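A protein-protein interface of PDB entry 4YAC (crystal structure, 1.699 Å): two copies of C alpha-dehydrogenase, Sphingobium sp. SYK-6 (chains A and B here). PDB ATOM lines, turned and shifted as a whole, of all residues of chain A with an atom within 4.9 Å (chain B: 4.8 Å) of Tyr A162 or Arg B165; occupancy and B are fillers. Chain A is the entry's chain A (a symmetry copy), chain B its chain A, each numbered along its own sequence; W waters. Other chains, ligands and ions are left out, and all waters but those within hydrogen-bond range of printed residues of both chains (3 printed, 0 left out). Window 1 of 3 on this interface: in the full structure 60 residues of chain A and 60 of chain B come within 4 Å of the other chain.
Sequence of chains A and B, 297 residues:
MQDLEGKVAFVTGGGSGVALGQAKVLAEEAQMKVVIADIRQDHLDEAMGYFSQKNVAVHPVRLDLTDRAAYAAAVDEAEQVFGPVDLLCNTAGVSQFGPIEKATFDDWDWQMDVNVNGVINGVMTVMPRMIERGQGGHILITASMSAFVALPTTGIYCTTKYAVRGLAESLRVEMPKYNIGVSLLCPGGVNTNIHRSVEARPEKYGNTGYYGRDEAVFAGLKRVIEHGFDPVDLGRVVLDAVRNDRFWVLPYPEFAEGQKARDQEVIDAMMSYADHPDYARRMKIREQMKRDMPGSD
The side-chain carboxylate of Glu B169 sits at hydrogen-bond distance from the side-chain hydroxyl of Tyr A162, at 2.8 Å.
The backbone carbonyl oxygen of Ala B147 sits at hydrogen-bond distance from the guanidinium group of Arg B165 (3.0 Å).
The backbone carbonyl oxygen (O) of Phe B148 sits at hydrogen-bond distance from the side-chain hydroxyl (OH) of Tyr B162 (3.3 Å).
The side-chain carboxylate of Glu B169 is in salt-bridge range of the guanidinium group of Arg B165, 2.9 Å away.
SG of Cys A158 lies within hydrogen-bond range of O of Ser A146 (3.4 Å).
The backbone carbonyl oxygen (O) of Ala A147 sits at hydrogen-bond distance from the guanidinium group (NH1) of Arg A165, 3.0 Å away.
The side-chain hydroxyl of Tyr A162 is in hydrogen-bond range of the backbone carbonyl oxygen of Phe A148.
Gly B166 touches Cys A158 (O to SG, 3.8 Å).
Thr A159 touches Ala B163.
Thr A159 touches Leu B167.
Tyr A162 touches Tyr B162.
Arg B165 touches Tyr A162.
CG of Tyr A162 touches CA of Gly B166, 3.5 Å away.
CB of Ala A163 touches CB of Ala B163 (3.9 Å).
Arg A165 touches Tyr B162 (NE to CE2, 3.6 Å).
CA of Gly A166 touches CG of Tyr B162, 3.5 Å away.
Ala A147 touches none of the printed residues of chain B.
Of the printed residues of chain B, Thr A159 touches Ala B163 and Leu B167.
Printed residues of chain B within 4 Å of Ala A163: Ala B163 (3.9 Å).
Printed residues of chain B within 4 Å of Arg A165: Tyr B162 (3.6 Å).
Of chain A, only Tyr A162 (3.6 Å) comes within 4 Å of Arg B165.
The nearest printed residue of chain B that does not touch Thr A159 is Gly B166 (4.1 Å).
Of the 13 printed residues of chain B, 6 touch a printed residue of chain A.
Hydrophobic or aromatic side chains of chain B that line the printed part of chain A: Tyr B162, Ala B163 and Leu B167.
Along chain B the printed residues that touch a printed residue of chain A span positions 162 to 169.
Of the 13 printed residues of chain A, 6 touch a printed residue of chain B.
Printed residues of chain A that touch a printed residue of chain B: Cys A158, Thr A159, Tyr A162, Ala A163, Arg A165 and Gly A166.
Among the printed residues, 10 pairs touch across the chains.
Tyr B162 touches its own counterpart, Tyr A162.
Tyr A162 touches Arg B165, and with the chains exchanged Arg A165 touches Tyr B162.
Tyr A162 touches Gly B166, and with the chains exchanged Gly A166 touches Tyr B162.
Ala A163 touches its own counterpart, Ala B163.
Positions printed for both chains: 147, 148, 161, 162, 163, 164, 165 and 166.
Of the 10 pairs that touch across the chains among the printed residues, 6 have their exchanged pair printed and touching as well.
Water W1 lies within hydrogen-bond range of the side-chain carboxylate of Glu B169 (2.7 Å), the backbone carbonyl oxygen of Phe A148 (2.8 Å) and the side-chain hydroxyl of Tyr A162 (3.4 Å).
Water W2 bridges the guanidinium group of Arg A165 (3.0 Å) and the guanidinium group of Arg B165 (3.0 Å).
Water W3 lies within hydrogen-bond range of the guanidinium group (NH2) of Arg B165 (3.0 Å) and the guanidinium group (NH1) of Arg A165 (3.0 Å).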
ATOM      1  N   SER A 146       4.122  21.594  21.388  1.00  0.00           N
ATOM      2  CA  SER A 146       4.434  20.184  21.607  1.00  0.00           C
ATOM      3  C   SER A 146       3.336  19.282  21.050  1.00  0.00           C
ATOM      4  O   SER A 146       3.472  18.061  21.055  1.00  0.00           O
ATOM      5  CB  SER A 146       4.631  19.897  23.096  1.00  0.00           C
ATOM      6  OG  SER A 146       5.838  20.465  23.564  1.00  0.00           O
ATOM      7  N   ALA A 147       2.242  19.885  20.588  1.00  0.00           N
ATOM      8  CA  ALA A 147       1.209  19.147  19.875  1.00  0.00           C
ATOM      9  C   ALA A 147       1.622  18.929  18.416  1.00  0.00           C
ATOM     10  O   ALA A 147       0.889  18.307  17.647  1.00  0.00           O
ATOM     11  CB  ALA A 147      -0.120  19.884  19.948  1.00  0.00           C
ATOM     12  N   PHE A 148       2.790  19.453  18.043  1.00  0.00           N
ATOM     13  CA  PHE A 148       3.329  19.302  16.692  1.00  0.00           C
ATOM     14  C   PHE A 148       4.761  18.778  16.685  1.00  0.00           C
ATOM     15  O   PHE A 148       5.215  18.220  15.684  1.00  0.00           O
ATOM     16  CB  PHE A 148       3.305  20.634  15.945  1.00  0.00           C
ATOM     17  CG  PHE A 148       1.936  21.068  15.520  1.00  0.00           C
ATOM     18  CD1 PHE A 148       1.412  20.652  14.308  1.00  0.00           C
ATOM     19  CD2 PHE A 148       1.179  21.901  16.322  1.00  0.00           C
ATOM     20  CE1 PHE A 148       0.153  21.052  13.908  1.00  0.00           C
ATOM     21  CE2 PHE A 148      -0.079  22.305  15.929  1.00  0.00           C
ATOM     22  CZ  PHE A 148      -0.592  21.879  14.720  1.00  0.00           C
ATOM     23  N   VAL A 149       5.474  18.983  17.788  1.00  0.00           N
ATOM     24  CA  VAL A 149       6.910  18.721  17.827  1.00  0.00           C
ATOM     25  C   VAL A 149       7.338  17.968  19.074  1.00  0.00           C
ATOM     26  O   VAL A 149       7.301  18.503  20.181  1.00  0.00           O
ATOM     27  CB  VAL A 149       7.717  20.031  17.755  1.00  0.00           C
ATOM     28  CG1 VAL A 149       9.200  19.732  17.543  1.00  0.00           C
ATOM     29  CG2 VAL A 149       7.190  20.921  16.644  1.00  0.00           C
ATOM     30  N   CYS A 158       4.304  15.914  25.696  1.00  0.00           N
ATOM     31  CA  CYS A 158       3.966  15.854  24.279  1.00  0.00           C
ATOM     32  C   CYS A 158       2.762  14.953  24.039  1.00  0.00           C
ATOM     33  O   CYS A 158       1.857  15.303  23.277  1.00  0.00           O
ATOM     34  CB  CYS A 158       5.178  15.360  23.482  1.00  0.00           C
ATOM     35  SG  CYS A 158       4.891  15.050  21.727  1.00  0.00           S
ATOM     36  N   THR A 159       2.745  13.800  24.701  1.00  0.00           N
ATOM     37  CA  THR A 159       1.629  12.874  24.574  1.00  0.00           C
ATOM     38  C   THR A 159       0.321  13.570  24.965  1.00  0.00           C
ATOM     39  O   THR A 159      -0.672  13.456  24.251  1.00  0.00           O
ATOM     40  CB  THR A 159       1.829  11.615  25.435  1.00  0.00           C
ATOM     41  OG1 THR A 159       3.028  10.947  25.021  1.00  0.00           O
ATOM     42  CG2 THR A 159       0.663  10.658  25.262  1.00  0.00           C
ATOM     43  N   THR A 160       0.329  14.311  26.072  1.00  0.00           N
ATOM     44  CA  THR A 160      -0.896  14.973  26.536  1.00  0.00           C
ATOM     45  C   THR A 160      -1.352  16.077  25.592  1.00  0.00           C
ATOM     46  O   THR A 160      -2.549  16.302  25.436  1.00  0.00           O
ATOM     47  CB  THR A 160      -0.754  15.591  27.958  1.00  0.00           C
ATOM     48  OG1 THR A 160       0.135  16.717  27.943  1.00  0.00           O
ATOM     49  CG2 THR A 160      -0.279  14.555  28.969  1.00  0.00           C
ATOM     50  N   LYS A 161      -0.414  16.766  24.956  1.00  0.00           N
ATOM     51  CA  LYS A 161      -0.780  17.899  24.118  1.00  0.00           C
ATOM     52  C   LYS A 161      -1.250  17.426  22.744  1.00  0.00           C
ATOM     53  O   LYS A 161      -2.146  18.027  22.149  1.00  0.00           O
ATOM     54  CB  LYS A 161       0.394  18.878  24.011  1.00  0.00           C
ATOM     55  CG  LYS A 161       0.744  19.544  25.350  1.00  0.00           C
ATOM     56  CD  LYS A 161      -0.425  20.348  25.921  1.00  0.00           C
ATOM     57  CE  LYS A 161      -0.103  20.967  27.271  1.00  0.00           C
ATOM     58  NZ  LYS A 161      -1.276  21.718  27.812  1.00  0.00           N
ATOM     59  N   TYR A 162      -0.681  16.333  22.249  1.00  0.00           N
ATOM     60  CA  TYR A 162      -1.223  15.702  21.055  1.00  0.00           C
ATOM     61  C   TYR A 162      -2.668  15.287  21.319  1.00  0.00           C
ATOM     62  O   TYR A 162      -3.548  15.492  20.482  1.00  0.00           O
ATOM     63  CB  TYR A 162      -0.385  14.486  20.651  1.00  0.00           C
ATOM     64  CG  TYR A 162       0.641  14.775  19.581  1.00  0.00           C
ATOM     65  CD1 TYR A 162       1.828  15.426  19.891  1.00  0.00           C
ATOM     66  CD2 TYR A 162       0.437  14.381  18.265  1.00  0.00           C
ATOM     67  CE1 TYR A 162       2.770  15.687  18.923  1.00  0.00           C
ATOM     68  CE2 TYR A 162       1.374  14.638  17.291  1.00  0.00           C
ATOM     69  CZ  TYR A 162       2.538  15.292  17.625  1.00  0.00           C
ATOM     70  OH  TYR A 162       3.472  15.546  16.651  1.00  0.00           O
ATOM     71  N   ALA A 163      -2.910  14.729  22.500  1.00  0.00           N
ATOM     72  CA  ALA A 163      -4.241  14.256  22.859  1.00  0.00           C
ATOM     73  C   ALA A 163      -5.283  15.362  22.745  1.00  0.00           C
ATOM     74  O   ALA A 163      -6.294  15.186  22.071  1.00  0.00           O
ATOM     75  CB  ALA A 163      -4.240  13.685  24.267  1.00  0.00           C
ATOM     76  N   VAL A 164      -5.044  16.501  23.385  1.00  0.00           N
ATOM     77  CA  VAL A 164      -6.058  17.552  23.393  1.00  0.00           C
ATOM     78  C   VAL A 164      -6.113  18.246  22.037  1.00  0.00           C
ATOM     79  O   VAL A 164      -7.136  18.830  21.691  1.00  0.00           O
ATOM     80  CB  VAL A 164      -5.827  18.585  24.516  1.00  0.00           C
ATOM     81  CG1 VAL A 164      -6.020  17.924  25.876  1.00  0.00           C
ATOM     82  CG2 VAL A 164      -4.460  19.230  24.407  1.00  0.00           C
ATOM     83  N   ARG A 165      -5.042  18.166  21.252  1.00  0.00           N
ATOM     84  CA  ARG A 165      -5.118  18.636  19.871  1.00  0.00           C
ATOM     85  C   ARG A 165      -6.153  17.809  19.121  1.00  0.00           C
ATOM     86  O   ARG A 165      -6.974  18.349  18.385  1.00  0.00           O
ATOM     87  CB  ARG A 165      -3.767  18.550  19.159  1.00  0.00           C
ATOM     88  CG  ARG A 165      -3.886  18.703  17.646  1.00  0.00           C
ATOM     89  CD  ARG A 165      -2.556  18.611  16.936  1.00  0.00           C
ATOM     90  NE  ARG A 165      -2.742  18.533  15.488  1.00  0.00           N
ATOM     91  CZ  ARG A 165      -1.794  18.193  14.622  1.00  0.00           C
ATOM     92  NH1 ARG A 165      -0.576  17.891  15.049  1.00  0.00           N
ATOM     93  NH2 ARG A 165      -2.067  18.146  13.325  1.00  0.00           N
ATOM     94  N   GLY A 166      -6.100  16.494  19.306  1.00  0.00           N
ATOM     95  CA  GLY A 166      -7.053  15.597  18.678  1.00  0.00           C
ATOM     96  C   GLY A 166      -8.466  15.931  19.107  1.00  0.00           C
ATOM     97  O   GLY A 166      -9.392  15.970  18.290  1.00  0.00           O
ATOM     98  N   ALA B 147      -5.360   9.422  13.755  1.00  0.00           N
ATOM     99  CA  ALA B 147      -4.291  10.207  14.359  1.00  0.00           C
ATOM    100  C   ALA B 147      -3.942  11.404  13.470  1.00  0.00           C
ATOM    101  O   ALA B 147      -3.071  12.203  13.816  1.00  0.00           O
ATOM    102  CB  ALA B 147      -3.063   9.341  14.595  1.00  0.00           C
ATOM    103  N   PHE B 148      -4.617  11.513  12.326  1.00  0.00           N
ATOM    104  CA  PHE B 148      -4.414  12.619  11.390  1.00  0.00           C
ATOM    105  C   PHE B 148      -5.717  13.308  11.001  1.00  0.00           C
ATOM    106  O   PHE B 148      -5.706  14.463  10.570  1.00  0.00           O
ATOM    107  CB  PHE B 148      -3.732  12.130  10.113  1.00  0.00           C
ATOM    108  CG  PHE B 148      -2.281  11.803  10.285  1.00  0.00           C
ATOM    109  CD1 PHE B 148      -1.317  12.784  10.139  1.00  0.00           C
ATOM    110  CD2 PHE B 148      -1.880  10.512  10.578  1.00  0.00           C
ATOM    111  CE1 PHE B 148       0.022  12.487  10.293  1.00  0.00           C
ATOM    112  CE2 PHE B 148      -0.545  10.209  10.731  1.00  0.00           C
ATOM    113  CZ  PHE B 148       0.408  11.198  10.589  1.00  0.00           C
ATOM    114  N   LYS B 161      -6.018   8.282  19.597  1.00  0.00           N
ATOM    115  CA  LYS B 161      -5.047   7.927  18.572  1.00  0.00           C
ATOM    116  C   LYS B 161      -4.057   9.067  18.345  1.00  0.00           C
ATOM    117  O   LYS B 161      -2.880   8.828  18.072  1.00  0.00           O
ATOM    118  CB  LYS B 161      -5.767   7.532  17.277  1.00  0.00           C
ATOM    119  CG  LYS B 161      -6.597   6.248  17.420  1.00  0.00           C
ATOM    120  CD  LYS B 161      -5.740   5.044  17.810  1.00  0.00           C
ATOM    121  CE  LYS B 161      -6.564   3.780  18.003  1.00  0.00           C
ATOM    122  NZ  LYS B 161      -5.700   2.633  18.414  1.00  0.00           N
ATOM    123  N   TYR B 162      -4.512  10.306  18.490  1.00  0.00           N
ATOM    124  CA  TYR B 162      -3.588  11.429  18.505  1.00  0.00           C
ATOM    125  C   TYR B 162      -2.603  11.253  19.657  1.00  0.00           C
ATOM    126  O   TYR B 162      -1.400  11.464  19.499  1.00  0.00           O
ATOM    127  CB  TYR B 162      -4.340  12.756  18.645  1.00  0.00           C
ATOM    128  CG  TYR B 162      -4.594  13.460  17.333  1.00  0.00           C
ATOM    129  CD1 TYR B 162      -5.604  13.035  16.481  1.00  0.00           C
ATOM    130  CD2 TYR B 162      -3.839  14.562  16.953  1.00  0.00           C
ATOM    131  CE1 TYR B 162      -5.844  13.677  15.287  1.00  0.00           C
ATOM    132  CE2 TYR B 162      -4.072  15.208  15.761  1.00  0.00           C
ATOM    133  CZ  TYR B 162      -5.075  14.761  14.932  1.00  0.00           C
ATOM    134  OH  TYR B 162      -5.308  15.409  13.744  1.00  0.00           O
ATOM    135  N   ALA B 163      -3.118  10.838  20.810  1.00  0.00           N
ATOM    136  CA  ALA B 163      -2.289  10.667  21.995  1.00  0.00           C
ATOM    137  C   ALA B 163      -1.127   9.715  21.738  1.00  0.00           C
ATOM    138  O   ALA B 163       0.023  10.069  21.987  1.00  0.00           O
ATOM    139  CB  ALA B 163      -3.125  10.164  23.160  1.00  0.00           C
ATOM    140  N   VAL B 164      -1.410   8.519  21.234  1.00  0.00           N
ATOM    141  CA  VAL B 164      -0.344   7.535  21.069  1.00  0.00           C
ATOM    142  C   VAL B 164       0.538   7.902  19.881  1.00  0.00           C
ATOM    143  O   VAL B 164       1.691   7.486  19.824  1.00  0.00           O
ATOM    144  CB  VAL B 164      -0.888   6.099  20.910  1.00  0.00           C
ATOM    145  CG1 VAL B 164      -1.557   5.653  22.205  1.00  0.00           C
ATOM    146  CG2 VAL B 164      -1.838   5.990  19.734  1.00  0.00           C
ATOM    147  N   ARG B 165       0.023   8.699  18.946  1.00  0.00           N
ATOM    148  CA  ARG B 165       0.887   9.241  17.901  1.00  0.00           C
ATOM    149  C   ARG B 165       1.957  10.114  18.543  1.00  0.00           C
ATOM    150  O   ARG B 165       3.130  10.026  18.193  1.00  0.00           O
ATOM    151  CB  ARG B 165       0.102  10.054  16.871  1.00  0.00           C
ATOM    152  CG  ARG B 165       1.002  10.905  15.979  1.00  0.00           C
ATOM    153  CD  ARG B 165       0.231  11.716  14.964  1.00  0.00           C
ATOM    154  NE  ARG B 165       1.105  12.678  14.295  1.00  0.00           N
ATOM    155  CZ  ARG B 165       0.681  13.691  13.548  1.00  0.00           C
ATOM    156  NH1 ARG B 165      -0.617  13.890  13.367  1.00  0.00           N
ATOM    157  NH2 ARG B 165       1.557  14.512  12.986  1.00  0.00           N
ATOM    158  N   GLY B 166       1.540  10.961  19.479  1.00  0.00           N
ATOM    159  CA  GLY B 166       2.465  11.821  20.193  1.00  0.00           C
ATOM    160  C   GLY B 166       3.499  10.999  20.934  1.00  0.00           C
ATOM    161  O   GLY B 166       4.695  11.308  20.918  1.00  0.00           O
ATOM    162  N   LEU B 167       3.030   9.949  21.598  1.00  0.00           N
ATOM    163  CA  LEU B 167       3.921   9.056  22.328  1.00  0.00           C
ATOM    164  C   LEU B 167       4.922   8.415  21.375  1.00  0.00           C
ATOM    165  O   LEU B 167       6.110   8.313  21.685  1.00  0.00           O
ATOM    166  CB  LEU B 167       3.130   7.972  23.063  1.00  0.00           C
ATOM    167  CG  LEU B 167       3.971   6.887  23.746  1.00  0.00           C
ATOM    168  CD1 LEU B 167       4.940   7.483  24.755  1.00  0.00           C
ATOM    169  CD2 LEU B 167       3.065   5.872  24.421  1.00  0.00           C
ATOM    170  N   ALA B 168       4.439   7.988  20.213  1.00  0.00           N
ATOM    171  CA  ALA B 168       5.305   7.359  19.219  1.00  0.00           C
ATOM    172  C   ALA B 168       6.380   8.325  18.726  1.00  0.00           C
ATOM    173  O   ALA B 168       7.559   7.964  18.646  1.00  0.00           O
ATOM    174  CB  ALA B 168       4.484   6.841  18.048  1.00  0.00           C
ATOM    175  N   GLU B 169       5.982   9.550  18.392  1.00  0.00           N
ATOM    176  CA  GLU B 169       6.940  10.539  17.909  1.00  0.00           C
ATOM    177  C   GLU B 169       7.934  10.904  19.012  1.00  0.00           C
ATOM    178  O   GLU B 169       9.078  11.268  18.731  1.00  0.00           O
ATOM    179  CB  GLU B 169       6.219  11.790  17.400  1.00  0.00           C
ATOM    180  CG  GLU B 169       5.352  11.533  16.182  1.00  0.00           C
ATOM    181  CD  GLU B 169       4.949  12.809  15.472  1.00  0.00           C
ATOM    182  OE1 GLU B 169       5.850  13.553  15.027  1.00  0.00           O
ATOM    183  OE2 GLU B 169       3.729  13.071  15.360  1.00  0.00           O
ATOM    184  N   LEU B 184       5.344   3.515  13.765  1.00  0.00           N
ATOM    185  CA  LEU B 184       3.970   3.940  13.980  1.00  0.00           C
ATOM    186  C   LEU B 184       3.117   3.534  12.786  1.00  0.00           C
ATOM    187  O   LEU B 184       3.234   4.106  11.702  1.00  0.00           O
ATOM    188  CB  LEU B 184       3.899   5.455  14.201  1.00  0.00           C
ATOM    189  CG  LEU B 184       2.509   6.061  14.388  1.00  0.00           C
ATOM    190  CD1 LEU B 184       1.845   5.530  15.652  1.00  0.00           C
ATOM    191  CD2 LEU B 184       2.624   7.574  14.431  1.00  0.00           C
ATOM    192  N   TRP B 248       7.253   6.067   9.944  1.00  0.00           N
ATOM    193  CA  TRP B 248       5.934   6.335   9.376  1.00  0.00           C
ATOM    194  C   TRP B 248       5.448   5.169   8.524  1.00  0.00           C
ATOM    195  O   TRP B 248       5.868   5.016   7.379  1.00  0.00           O
ATOM    196  CB  TRP B 248       5.949   7.607   8.524  1.00  0.00           C
ATOM    197  CG  TRP B 248       6.172   8.870   9.292  1.00  0.00           C
ATOM    198  CD1 TRP B 248       7.231   9.724   9.173  1.00  0.00           C
ATOM    199  CD2 TRP B 248       5.316   9.431  10.295  1.00  0.00           C
ATOM    200  NE1 TRP B 248       7.086  10.780  10.038  1.00  0.00           N
ATOM    201  CE2 TRP B 248       5.919  10.623  10.741  1.00  0.00           C
ATOM    202  CE3 TRP B 248       4.097   9.042  10.860  1.00  0.00           C
ATOM    203  CZ2 TRP B 248       5.347  11.429  11.723  1.00  0.00           C
ATOM    204  CZ3 TRP B 248       3.531   9.843  11.836  1.00  0.00           C
ATOM    205  CH2 TRP B 248       4.157  11.022  12.257  1.00  0.00           C
HETATM  206  O   HOH W   1       6.802  15.891  15.925  1.00  0.00           O
HETATM  207  O   HOH W   2      -1.076  16.125  11.376  1.00  0.00           O
HETATM  208  O   HOH W   3       1.291  17.465  12.703  1.00  0.00           O
